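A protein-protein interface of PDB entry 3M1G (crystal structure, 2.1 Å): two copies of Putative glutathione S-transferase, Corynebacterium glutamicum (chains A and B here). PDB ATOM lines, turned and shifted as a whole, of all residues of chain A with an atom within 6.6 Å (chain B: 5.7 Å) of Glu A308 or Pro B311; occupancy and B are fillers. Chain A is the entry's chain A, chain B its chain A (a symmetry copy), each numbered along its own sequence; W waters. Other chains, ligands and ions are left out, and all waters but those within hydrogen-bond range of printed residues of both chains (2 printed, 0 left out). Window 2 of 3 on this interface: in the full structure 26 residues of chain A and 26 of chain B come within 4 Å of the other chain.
Of chain B, only Pro B311 comes within 4 Å of Glu A308.
Of the printed residues of chain B, Pro A311 touches Glu B308 (3.4 Å), Ile B309 (3.8 Å) and Pro B311 (3.4 Å).
Of the printed residues of chain A, Glu B308 touches Pro A311.
Of the printed residues of chain A, Ile B309 touches Ile A309 (3.9 Å) and Pro A311 (3.8 Å).
Pro B311 touches just these residues of chain A: Glu A308, Ile A309 and Pro A311.
The nearest printed residue of chain A that does not touch Ile B309 is Asn A310 (4.6 Å).
Water W1 lies within hydrogen-bond range of OD1 of Asn B310 (2.8 Å), O of Ile A309 (2.8 Å) and OG1 of Thr B312 (3.1 Å).
Water W2 bridges the side-chain amide oxygen (OD1) of Asn A310 and the backbone carbonyl oxygen (O) of Ile B309.
Glu A308 touches Pro B311.
O of Ile B309 touches O of Ile A309, at 3.9 Å.
Ile A309 touches Pro B311.
CG of Pro A311 touches O of Glu B308, 3.4 Å away.
O of Ile B309 touches CD of Pro A311, at 3.8 Å.
Pro A311 touches Pro B311 (CD to CD, 3.4 Å).
Glu A308 touches Pro B311, and with the chains exchanged Pro A311 touches Glu B308.
Ile B309 touches its own counterpart, Ile A309.
Ile A309 touches Pro B311, and with the chains exchanged Pro A311 touches Ile B309.
Pro B311 touches its own counterpart, Pro A311.
Positions printed for both chains: 306, 307, 308, 309, 310 and 311.
Of the 6 pairs that touch across the chains among the printed residues, 6 have their exchanged pair printed and touching as well.
Printed residues of chain A that touch a printed residue of chain B: Glu A308, Ile A309 and Pro A311.
Hydrophobic or aromatic side chains of chain A within 4 Å of the printed part of chain B: Pro A311.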
ATOM      1  N   THR A 305       8.425 -35.977 -18.463  1.00  0.00           N
ATOM      2  CA  THR A 305       7.687 -35.828 -19.720  1.00  0.00           C
ATOM      3  C   THR A 305       7.031 -34.478 -19.950  1.00  0.00           C
ATOM      4  O   THR A 305       6.933 -34.049 -21.085  1.00  0.00           O
ATOM      5  CB  THR A 305       6.602 -36.947 -19.741  1.00  0.00           C
ATOM      6  OG1 THR A 305       7.295 -38.172 -19.961  1.00  0.00           O
ATOM      7  CG2 THR A 305       5.502 -36.723 -20.749  1.00  0.00           C
ATOM      8  N   HIS A 306       6.563 -33.815 -18.892  1.00  0.00           N
ATOM      9  CA  HIS A 306       5.832 -32.565 -19.057  1.00  0.00           C
ATOM     10  C   HIS A 306       6.805 -31.392 -18.984  1.00  0.00           C
ATOM     11  O   HIS A 306       6.795 -30.584 -18.014  1.00  0.00           O
ATOM     12  CB  HIS A 306       4.726 -32.415 -18.013  1.00  0.00           C
ATOM     13  CG  HIS A 306       3.658 -33.456 -18.099  1.00  0.00           C
ATOM     14  ND1 HIS A 306       2.841 -33.773 -17.033  1.00  0.00           N
ATOM     15  CD2 HIS A 306       3.284 -34.273 -19.115  1.00  0.00           C
ATOM     16  CE1 HIS A 306       2.003 -34.730 -17.395  1.00  0.00           C
ATOM     17  NE2 HIS A 306       2.249 -35.048 -18.652  1.00  0.00           N
ATOM     18  N   ALA A 307       7.640 -31.307 -20.018  1.00  0.00           N
ATOM     19  CA  ALA A 307       8.690 -30.320 -20.120  1.00  0.00           C
ATOM     20  C   ALA A 307       8.155 -28.890 -20.281  1.00  0.00           C
ATOM     21  O   ALA A 307       8.837 -27.933 -19.914  1.00  0.00           O
ATOM     22  CB  ALA A 307       9.647 -30.686 -21.285  1.00  0.00           C
ATOM     23  N   GLU A 308       6.940 -28.735 -20.792  1.00  0.00           N
ATOM     24  CA  GLU A 308       6.309 -27.417 -20.846  1.00  0.00           C
ATOM     25  C   GLU A 308       5.938 -26.857 -19.452  1.00  0.00           C
ATOM     26  O   GLU A 308       5.831 -25.650 -19.305  1.00  0.00           O
ATOM     27  CB  GLU A 308       5.068 -27.415 -21.765  1.00  0.00           C
ATOM     28  CG  GLU A 308       4.324 -26.029 -21.861  1.00  0.00           C
ATOM     29  CD  GLU A 308       5.217 -24.843 -22.317  1.00  0.00           C
ATOM     30  OE1 GLU A 308       5.502 -24.840 -23.553  1.00  0.00           O
ATOM     31  OE2 GLU A 308       5.600 -23.923 -21.476  1.00  0.00           O
ATOM     32  N   ILE A 309       5.749 -27.726 -18.456  1.00  0.00           N
ATOM     33  CA  ILE A 309       5.499 -27.336 -17.062  1.00  0.00           C
ATOM     34  C   ILE A 309       6.775 -27.339 -16.195  1.00  0.00           C
ATOM     35  O   ILE A 309       6.970 -26.439 -15.351  1.00  0.00           O
ATOM     36  CB  ILE A 309       4.507 -28.305 -16.409  1.00  0.00           C
ATOM     37  CG1 ILE A 309       3.169 -28.280 -17.132  1.00  0.00           C
ATOM     38  CG2 ILE A 309       4.294 -27.971 -14.921  1.00  0.00           C
ATOM     39  CD1 ILE A 309       2.177 -29.276 -16.456  1.00  0.00           C
ATOM     40  N   ASN A 310       7.631 -28.343 -16.421  1.00  0.00           N
ATOM     41  CA  ASN A 310       8.862 -28.608 -15.657  1.00  0.00           C
ATOM     42  C   ASN A 310      10.082 -28.761 -16.576  1.00  0.00           C
ATOM     43  O   ASN A 310      10.587 -29.863 -16.749  1.00  0.00           O
ATOM     44  CB  ASN A 310       8.670 -29.899 -14.837  1.00  0.00           C
ATOM     45  CG  ASN A 310       9.816 -30.168 -13.838  1.00  0.00           C
ATOM     46  OD1 ASN A 310      10.328 -29.238 -13.186  1.00  0.00           O
ATOM     47  ND2 ASN A 310      10.207 -31.449 -13.700  1.00  0.00           N
ATOM     48  N   PRO A 311      10.596 -27.646 -17.133  1.00  0.00           N
ATOM     49  CA  PRO A 311      11.655 -27.752 -18.131  1.00  0.00           C
ATOM     50  C   PRO A 311      12.948 -28.369 -17.633  1.00  0.00           C
ATOM     51  O   PRO A 311      13.711 -28.884 -18.441  1.00  0.00           O
ATOM     52  CB  PRO A 311      11.902 -26.290 -18.556  1.00  0.00           C
ATOM     53  CG  PRO A 311      11.242 -25.458 -17.525  1.00  0.00           C
ATOM     54  CD  PRO A 311      10.077 -26.276 -17.061  1.00  0.00           C
ATOM     55  N   HIS B 306      10.935 -16.735 -11.681  1.00  0.00           N
ATOM     56  CA  HIS B 306      11.844 -17.832 -11.987  1.00  0.00           C
ATOM     57  C   HIS B 306      11.282 -18.653 -13.145  1.00  0.00           C
ATOM     58  O   HIS B 306      10.861 -19.831 -12.976  1.00  0.00           O
ATOM     59  CB  HIS B 306      12.093 -18.719 -10.767  1.00  0.00           C
ATOM     60  CG  HIS B 306      12.763 -18.020  -9.629  1.00  0.00           C
ATOM     61  ND1 HIS B 306      12.684 -18.473  -8.329  1.00  0.00           N
ATOM     62  CD2 HIS B 306      13.506 -16.886  -9.588  1.00  0.00           C
ATOM     63  CE1 HIS B 306      13.360 -17.655  -7.540  1.00  0.00           C
ATOM     64  NE2 HIS B 306      13.870 -16.687  -8.279  1.00  0.00           N
ATOM     65  N   ALA B 307      11.282 -18.020 -14.316  1.00  0.00           N
ATOM     66  CA  ALA B 307      10.729 -18.580 -15.528  1.00  0.00           C
ATOM     67  C   ALA B 307      11.521 -19.789 -16.046  1.00  0.00           C
ATOM     68  O   ALA B 307      10.961 -20.640 -16.737  1.00  0.00           O
ATOM     69  CB  ALA B 307      10.626 -17.480 -16.618  1.00  0.00           C
ATOM     70  N   GLU B 308      12.798 -19.891 -15.697  1.00  0.00           N
ATOM     71  CA  GLU B 308      13.577 -21.082 -16.033  1.00  0.00           C
ATOM     72  C   GLU B 308      13.128 -22.346 -15.262  1.00  0.00           C
ATOM     73  O   GLU B 308      13.360 -23.447 -15.738  1.00  0.00           O
ATOM     74  CB  GLU B 308      15.090 -20.849 -15.835  1.00  0.00           C
ATOM     75  CG  GLU B 308      15.995 -22.098 -16.163  1.00  0.00           C
ATOM     76  CD  GLU B 308      15.817 -22.669 -17.597  1.00  0.00           C
ATOM     77  OE1 GLU B 308      16.348 -21.971 -18.513  1.00  0.00           O
ATOM     78  OE2 GLU B 308      15.194 -23.795 -17.802  1.00  0.00           O
ATOM     79  N   ILE B 309      12.498 -22.181 -14.097  1.00  0.00           N
ATOM     80  CA  ILE B 309      11.923 -23.280 -13.311  1.00  0.00           C
ATOM     81  C   ILE B 309      10.413 -23.478 -13.561  1.00  0.00           C
ATOM     82  O   ILE B 309       9.929 -24.626 -13.640  1.00  0.00           O
ATOM     83  CB  ILE B 309      12.101 -23.011 -11.812  1.00  0.00           C
ATOM     84  CG1 ILE B 309      13.574 -22.919 -11.448  1.00  0.00           C
ATOM     85  CG2 ILE B 309      11.428 -24.106 -10.962  1.00  0.00           C
ATOM     86  CD1 ILE B 309      13.733 -22.640  -9.921  1.00  0.00           C
ATOM     87  N   ASN B 310       9.693 -22.357 -13.693  1.00  0.00           N
ATOM     88  CA  ASN B 310       8.229 -22.292 -13.842  1.00  0.00           C
ATOM     89  C   ASN B 310       7.816 -21.446 -15.054  1.00  0.00           C
ATOM     90  O   ASN B 310       7.315 -20.341 -14.890  1.00  0.00           O
ATOM     91  CB  ASN B 310       7.626 -21.685 -12.560  1.00  0.00           C
ATOM     92  CG  ASN B 310       6.084 -21.756 -12.514  1.00  0.00           C
ATOM     93  OD1 ASN B 310       5.478 -22.767 -12.917  1.00  0.00           O
ATOM     94  ND2 ASN B 310       5.446 -20.687 -12.002  1.00  0.00           N
ATOM     95  N   PRO B 311       7.978 -21.980 -16.282  1.00  0.00           N
ATOM     96  CA  PRO B 311       7.746 -21.164 -17.467  1.00  0.00           C
ATOM     97  C   PRO B 311       6.326 -20.656 -17.630  1.00  0.00           C
ATOM     98  O   PRO B 311       6.126 -19.657 -18.311  1.00  0.00           O
ATOM     99  CB  PRO B 311       8.101 -22.108 -18.634  1.00  0.00           C
ATOM    100  CG  PRO B 311       8.149 -23.466 -18.048  1.00  0.00           C
ATOM    101  CD  PRO B 311       8.604 -23.259 -16.637  1.00  0.00           C
ATOM    102  N   THR B 312       5.331 -21.336 -17.060  1.00  0.00           N
ATOM    103  CA  THR B 312       3.953 -20.860 -17.217  1.00  0.00           C
ATOM    104  C   THR B 312       3.772 -19.580 -16.416  1.00  0.00           C
ATOM    105  O   THR B 312       2.863 -18.819 -16.665  1.00  0.00           O
ATOM    106  CB  THR B 312       2.912 -21.880 -16.722  1.00  0.00           C
ATOM    107  OG1 THR B 312       3.126 -22.119 -15.328  1.00  0.00           O
ATOM    108  CG2 THR B 312       2.974 -23.203 -17.570  1.00  0.00           C
ATOM    109  N   ARG B 313       4.645 -19.353 -15.438  1.00  0.00           N
ATOM    110  CA  ARG B 313       4.508 -18.215 -14.527  1.00  0.00           C
ATOM    111  C   ARG B 313       3.199 -18.147 -13.720  1.00  0.00           C
ATOM    112  O   ARG B 313       2.825 -17.083 -13.211  1.00  0.00           O
ATOM    113  CB  ARG B 313       4.731 -16.887 -15.275  1.00  0.00           C
ATOM    114  CG  ARG B 313       6.076 -16.801 -15.947  1.00  0.00           C
ATOM    115  CD  ARG B 313       6.408 -15.348 -16.344  1.00  0.00           C
ATOM    116  NE  ARG B 313       6.684 -15.326 -17.743  1.00  0.00           N
ATOM    117  CZ  ARG B 313       7.834 -15.014 -18.339  1.00  0.00           C
ATOM    118  NH1 ARG B 313       8.906 -14.625 -17.657  1.00  0.00           N
ATOM    119  NH2 ARG B 313       7.881 -15.082 -19.677  1.00  0.00           N
HETATM  120  O   HOH W   1       5.637 -23.971 -15.406  1.00  0.00           O
HETATM  121  O   HOH W   2      11.476 -26.910 -14.152  1.00  0.00           O
